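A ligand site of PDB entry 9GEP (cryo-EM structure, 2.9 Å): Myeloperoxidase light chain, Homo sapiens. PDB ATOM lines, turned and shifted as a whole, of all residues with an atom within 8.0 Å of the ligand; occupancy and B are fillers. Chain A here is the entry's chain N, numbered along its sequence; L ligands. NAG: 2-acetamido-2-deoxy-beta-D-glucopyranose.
OD1 of Asn 77 sits close to N of Ser 79 (3.4 Å).
The backbone NH (N) of Asn 77 sits at hydrogen-bond distance from the backbone carbonyl oxygen (O) of Leu 84, at 2.7 Å.
OD1 of Asn 80 lies within hydrogen-bond range of N of Leu 82 (2.9 Å).
The side-chain amide oxygen of Gln 89 lies within hydrogen-bond range of an oxygen (O3) of the ligand, 2.6 Å away.
The side-chain amide oxygen of Asn 77 lies close to an oxygen (O7) of the ligand (3.3 Å).
Merely in contact with the ligand: Ser 79 (3.7 Å) and Asn 80 (3.96 Å).
Four residues have an atom within 4 Å of the ligand: Asn 77, Ser 79, Asn 80 and Gln 89.
The nearest printed residue that does not touch the ligand is Val 87 (4.03 Å).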
ATOM      1  N   ASN A  74     -30.303  10.403  32.878  1.00  0.00           N
ATOM      2  CA  ASN A  74     -29.182   9.641  32.341  1.00  0.00           C
ATOM      3  C   ASN A  74     -28.649  10.203  31.024  1.00  0.00           C
ATOM      4  O   ASN A  74     -27.533   9.862  30.635  1.00  0.00           O
ATOM      5  CB  ASN A  74     -29.581   8.186  32.147  1.00  0.00           C
ATOM      6  CG  ASN A  74     -29.832   7.464  33.460  1.00  0.00           C
ATOM      7  OD1 ASN A  74     -29.479   7.964  34.531  1.00  0.00           O
ATOM      8  ND2 ASN A  74     -30.458   6.294  33.388  1.00  0.00           N
ATOM      9  N   LEU A  75     -29.418  11.043  30.342  1.00  0.00           N
ATOM     10  CA  LEU A  75     -28.974  11.639  29.083  1.00  0.00           C
ATOM     11  C   LEU A  75     -28.166  12.909  29.273  1.00  0.00           C
ATOM     12  O   LEU A  75     -27.645  13.444  28.292  1.00  0.00           O
ATOM     13  CB  LEU A  75     -30.187  11.942  28.196  1.00  0.00           C
ATOM     14  CG  LEU A  75     -30.477  10.971  27.055  1.00  0.00           C
ATOM     15  CD1 LEU A  75     -31.909  11.134  26.566  1.00  0.00           C
ATOM     16  CD2 LEU A  75     -29.494  11.177  25.921  1.00  0.00           C
ATOM     17  N   ARG A  76     -28.028  13.390  30.510  1.00  0.00           N
ATOM     18  CA  ARG A  76     -27.328  14.638  30.800  1.00  0.00           C
ATOM     19  C   ARG A  76     -25.875  14.363  31.165  1.00  0.00           C
ATOM     20  O   ARG A  76     -25.450  13.225  31.353  1.00  0.00           O
ATOM     21  CB  ARG A  76     -28.036  15.388  31.927  1.00  0.00           C
ATOM     22  CG  ARG A  76     -29.382  15.974  31.552  1.00  0.00           C
ATOM     23  CD  ARG A  76     -30.105  16.496  32.778  1.00  0.00           C
ATOM     24  NE  ARG A  76     -29.319  17.476  33.507  1.00  0.00           N
ATOM     25  CZ  ARG A  76     -29.788  18.263  34.464  1.00  0.00           C
ATOM     26  NH1 ARG A  76     -31.056  18.205  34.836  1.00  0.00           N
ATOM     27  NH2 ARG A  76     -28.974  19.124  35.056  1.00  0.00           N
ATOM     28  N   ASN A  77     -25.109  15.452  31.278  1.00  0.00           N
ATOM     29  CA  ASN A  77     -23.701  15.402  31.675  1.00  0.00           C
ATOM     30  C   ASN A  77     -23.599  15.901  33.104  1.00  0.00           C
ATOM     31  O   ASN A  77     -23.679  17.110  33.359  1.00  0.00           O
ATOM     32  CB  ASN A  77     -22.838  16.218  30.725  1.00  0.00           C
ATOM     33  CG  ASN A  77     -21.383  15.806  30.750  1.00  0.00           C
ATOM     34  OD1 ASN A  77     -20.934  15.153  31.687  1.00  0.00           O
ATOM     35  ND2 ASN A  77     -20.649  16.180  29.710  1.00  0.00           N
ATOM     36  N   MET A  78     -23.423  14.977  34.047  1.00  0.00           N
ATOM     37  CA  MET A  78     -23.355  15.295  35.476  1.00  0.00           C
ATOM     38  C   MET A  78     -21.924  15.418  35.978  1.00  0.00           C
ATOM     39  O   MET A  78     -21.717  15.599  37.185  1.00  0.00           O
ATOM     40  CB  MET A  78     -24.096  14.233  36.287  1.00  0.00           C
ATOM     41  CG  MET A  78     -25.592  14.027  35.945  1.00  0.00           C
ATOM     42  SD  MET A  78     -26.758  15.370  36.284  1.00  0.00           S
ATOM     43  CE  MET A  78     -26.452  16.563  34.986  1.00  0.00           C
ATOM     44  N   SER A  79     -20.932  15.337  35.092  1.00  0.00           N
ATOM     45  CA  SER A  79     -19.532  15.473  35.480  1.00  0.00           C
ATOM     46  C   SER A  79     -19.039  16.911  35.438  1.00  0.00           C
ATOM     47  O   SER A  79     -17.884  17.161  35.779  1.00  0.00           O
ATOM     48  CB  SER A  79     -18.653  14.594  34.591  1.00  0.00           C
ATOM     49  OG  SER A  79     -18.962  13.222  34.747  1.00  0.00           O
ATOM     50  N   ASN A  80     -19.889  17.854  35.018  1.00  0.00           N
ATOM     51  CA  ASN A  80     -19.517  19.261  34.975  1.00  0.00           C
ATOM     52  C   ASN A  80     -20.779  20.093  35.205  1.00  0.00           C
ATOM     53  O   ASN A  80     -21.816  19.572  35.607  1.00  0.00           O
ATOM     54  CB  ASN A  80     -18.768  19.568  33.657  1.00  0.00           C
ATOM     55  CG  ASN A  80     -19.681  19.678  32.436  1.00  0.00           C
ATOM     56  OD1 ASN A  80     -20.898  19.826  32.526  1.00  0.00           O
ATOM     57  ND2 ASN A  80     -19.061  19.604  31.260  1.00  0.00           N
ATOM     58  N   GLN A  81     -20.676  21.390  34.942  1.00  0.00           N
ATOM     59  CA  GLN A  81     -21.767  22.329  35.173  1.00  0.00           C
ATOM     60  C   GLN A  81     -22.025  23.177  33.937  1.00  0.00           C
ATOM     61  O   GLN A  81     -22.301  24.378  34.026  1.00  0.00           O
ATOM     62  CB  GLN A  81     -21.480  23.219  36.377  1.00  0.00           C
ATOM     63  CG  GLN A  81     -21.561  22.505  37.715  1.00  0.00           C
ATOM     64  CD  GLN A  81     -22.967  22.000  38.016  1.00  0.00           C
ATOM     65  OE1 GLN A  81     -23.267  20.821  37.819  1.00  0.00           O
ATOM     66  NE2 GLN A  81     -23.825  22.889  38.497  1.00  0.00           N
ATOM     67  N   LEU A  82     -21.942  22.565  32.752  1.00  0.00           N
ATOM     68  CA  LEU A  82     -22.219  23.255  31.504  1.00  0.00           C
ATOM     69  C   LEU A  82     -23.553  22.857  30.894  1.00  0.00           C
ATOM     70  O   LEU A  82     -23.934  23.412  29.850  1.00  0.00           O
ATOM     71  CB  LEU A  82     -21.095  23.009  30.492  1.00  0.00           C
ATOM     72  CG  LEU A  82     -19.671  22.954  31.049  1.00  0.00           C
ATOM     73  CD1 LEU A  82     -18.681  22.584  29.941  1.00  0.00           C
ATOM     74  CD2 LEU A  82     -19.297  24.282  31.689  1.00  0.00           C
ATOM     75  N   LEU A  84     -24.529  19.888  29.470  1.00  0.00           N
ATOM     76  CA  LEU A  84     -24.346  19.156  28.234  1.00  0.00           C
ATOM     77  C   LEU A  84     -25.082  17.818  28.286  1.00  0.00           C
ATOM     78  O   LEU A  84     -25.498  17.343  29.346  1.00  0.00           O
ATOM     79  CB  LEU A  84     -22.848  18.924  27.965  1.00  0.00           C
ATOM     80  CG  LEU A  84     -22.049  20.107  27.411  1.00  0.00           C
ATOM     81  CD1 LEU A  84     -20.816  19.631  26.681  1.00  0.00           C
ATOM     82  CD2 LEU A  84     -22.905  20.988  26.508  1.00  0.00           C
ATOM     83  N   LEU A  85     -25.244  17.219  27.108  1.00  0.00           N
ATOM     84  CA  LEU A  85     -25.841  15.887  26.999  1.00  0.00           C
ATOM     85  C   LEU A  85     -24.752  14.829  27.021  1.00  0.00           C
ATOM     86  O   LEU A  85     -23.651  15.039  26.487  1.00  0.00           O
ATOM     87  CB  LEU A  85     -26.661  15.772  25.714  1.00  0.00           C
ATOM     88  CG  LEU A  85     -28.015  16.484  25.654  1.00  0.00           C
ATOM     89  CD1 LEU A  85     -28.574  16.436  24.245  1.00  0.00           C
ATOM     90  CD2 LEU A  85     -28.986  15.886  26.643  1.00  0.00           C
ATOM     91  N   ALA A  86     -25.043  13.701  27.651  1.00  0.00           N
ATOM     92  CA  ALA A  86     -24.092  12.606  27.723  1.00  0.00           C
ATOM     93  C   ALA A  86     -23.691  12.164  26.316  1.00  0.00           C
ATOM     94  O   ALA A  86     -24.524  12.081  25.415  1.00  0.00           O
ATOM     95  CB  ALA A  86     -24.680  11.426  28.495  1.00  0.00           C
ATOM     96  N   VAL A  87     -22.399  11.896  26.142  1.00  0.00           N
ATOM     97  CA  VAL A  87     -21.824  11.606  24.841  1.00  0.00           C
ATOM     98  C   VAL A  87     -21.027  10.303  24.924  1.00  0.00           C
ATOM     99  O   VAL A  87     -20.982   9.648  25.960  1.00  0.00           O
ATOM    100  CB  VAL A  87     -20.955  12.766  24.321  1.00  0.00           C
ATOM    101  CG1 VAL A  87     -21.829  13.828  23.691  1.00  0.00           C
ATOM    102  CG2 VAL A  87     -20.120  13.345  25.456  1.00  0.00           C
ATOM    103  N   ASN A  88     -20.398   9.945  23.801  1.00  0.00           N
ATOM    104  CA  ASN A  88     -19.645   8.701  23.724  1.00  0.00           C
ATOM    105  C   ASN A  88     -18.264   8.875  24.325  1.00  0.00           C
ATOM    106  O   ASN A  88     -17.562   9.843  24.028  1.00  0.00           O
ATOM    107  CB  ASN A  88     -19.533   8.237  22.276  1.00  0.00           C
ATOM    108  CG  ASN A  88     -19.750   6.747  22.120  1.00  0.00           C
ATOM    109  OD1 ASN A  88     -18.918   5.941  22.545  1.00  0.00           O
ATOM    110  ND2 ASN A  88     -20.861   6.374  21.509  1.00  0.00           N
ATOM    111  N   GLN A  89     -17.872   7.935  25.184  1.00  0.00           N
ATOM    112  CA  GLN A  89     -16.572   7.959  25.851  1.00  0.00           C
ATOM    113  C   GLN A  89     -15.542   7.056  25.179  1.00  0.00           C
ATOM    114  O   GLN A  89     -14.412   6.972  25.660  1.00  0.00           O
ATOM    115  CB  GLN A  89     -16.730   7.550  27.319  1.00  0.00           C
ATOM    116  CG  GLN A  89     -17.601   8.495  28.128  1.00  0.00           C
ATOM    117  CD  GLN A  89     -17.089   9.912  28.121  1.00  0.00           C
ATOM    118  OE1 GLN A  89     -17.717  10.807  27.559  1.00  0.00           O
ATOM    119  NE2 GLN A  89     -15.941  10.131  28.752  1.00  0.00           N
ATOM    120  N   ARG A  90     -15.907   6.387  24.091  1.00  0.00           N
ATOM    121  CA  ARG A  90     -15.010   5.430  23.451  1.00  0.00           C
ATOM    122  C   ARG A  90     -14.681   5.768  22.007  1.00  0.00           C
ATOM    123  O   ARG A  90     -13.510   5.654  21.605  1.00  0.00           O
ATOM    124  CB  ARG A  90     -15.609   4.014  23.513  1.00  0.00           C
ATOM    125  CG  ARG A  90     -16.301   3.692  24.825  1.00  0.00           C
ATOM    126  CD  ARG A  90     -16.080   2.231  25.201  1.00  0.00           C
ATOM    127  NE  ARG A  90     -16.046   1.373  24.020  1.00  0.00           N
ATOM    128  CZ  ARG A  90     -16.839   0.334  23.831  1.00  0.00           C
ATOM    129  NH1 ARG A  90     -17.759  -0.012  24.720  1.00  0.00           N
ATOM    130  NH2 ARG A  90     -16.723  -0.382  22.710  1.00  0.00           N
ATOM    131  N   GLN A  92     -15.348   8.535  18.493  1.00  0.00           N
ATOM    132  CA  GLN A  92     -15.746   9.858  18.036  1.00  0.00           C
ATOM    133  C   GLN A  92     -15.758   9.859  16.504  1.00  0.00           C
ATOM    134  O   GLN A  92     -15.045   9.080  15.865  1.00  0.00           O
ATOM    135  CB  GLN A  92     -14.818  10.963  18.558  1.00  0.00           C
ATOM    136  CG  GLN A  92     -14.875  11.160  20.066  1.00  0.00           C
ATOM    137  CD  GLN A  92     -14.513  12.580  20.474  1.00  0.00           C
ATOM    138  OE1 GLN A  92     -13.589  13.176  19.919  1.00  0.00           O
ATOM    139  NE2 GLN A  92     -15.228  13.114  21.455  1.00  0.00           N
ATOM    140  N   PRO A 100     -24.136   7.973  23.673  1.00  0.00           N
ATOM    141  CA  PRO A 100     -23.617   6.941  24.579  1.00  0.00           C
ATOM    142  C   PRO A 100     -24.277   5.597  24.303  1.00  0.00           C
ATOM    143  O   PRO A 100     -25.416   5.509  23.835  1.00  0.00           O
ATOM    144  CB  PRO A 100     -23.989   7.471  25.970  1.00  0.00           C
ATOM    145  CG  PRO A 100     -25.135   8.389  25.735  1.00  0.00           C
ATOM    146  CD  PRO A 100     -24.915   8.999  24.386  1.00  0.00           C
ATOM    147  N   ASN A 146     -25.585  20.242  22.397  1.00  0.00           N
ATOM    148  CA  ASN A 146     -24.313  20.477  23.090  1.00  0.00           C
ATOM    149  C   ASN A 146     -23.662  21.777  22.629  1.00  0.00           C
ATOM    150  O   ASN A 146     -23.200  22.573  23.456  1.00  0.00           O
ATOM    151  CB  ASN A 146     -23.377  19.289  22.862  1.00  0.00           C
ATOM    152  CG  ASN A 146     -23.665  18.127  23.781  1.00  0.00           C
ATOM    153  OD1 ASN A 146     -24.664  18.124  24.501  1.00  0.00           O
ATOM    154  ND2 ASN A 146     -22.794  17.127  23.764  1.00  0.00           N
HETATM  155  C1  NAG L   1     -17.679  14.890  31.082  1.00  0.00           C
HETATM  156  C2  NAG L   1     -17.708  13.896  29.919  1.00  0.00           C
HETATM  157  C3  NAG L   1     -16.302  13.714  29.357  1.00  0.00           C
HETATM  158  C4  NAG L   1     -15.663  15.064  29.049  1.00  0.00           C
HETATM  159  C5  NAG L   1     -15.734  15.954  30.288  1.00  0.00           C
HETATM  160  C6  NAG L   1     -15.137  17.337  30.092  1.00  0.00           C
HETATM  161  C7  NAG L   1     -19.500  12.201  30.107  1.00  0.00           C
HETATM  162  C8  NAG L   1     -19.824  10.841  30.670  1.00  0.00           C
HETATM  163  N2  NAG L   1     -18.250  12.629  30.360  1.00  0.00           N
HETATM  164  O3  NAG L   1     -16.388  12.896  28.216  1.00  0.00           O
HETATM  165  O4  NAG L   1     -14.336  14.826  28.648  1.00  0.00           O
HETATM  166  O5  NAG L   1     -17.087  16.096  30.669  1.00  0.00           O
HETATM  167  O6  NAG L   1     -15.391  18.123  31.221  1.00  0.00           O
HETATM  168  O7  NAG L   1     -20.313  12.847  29.462  1.00  0.00           O
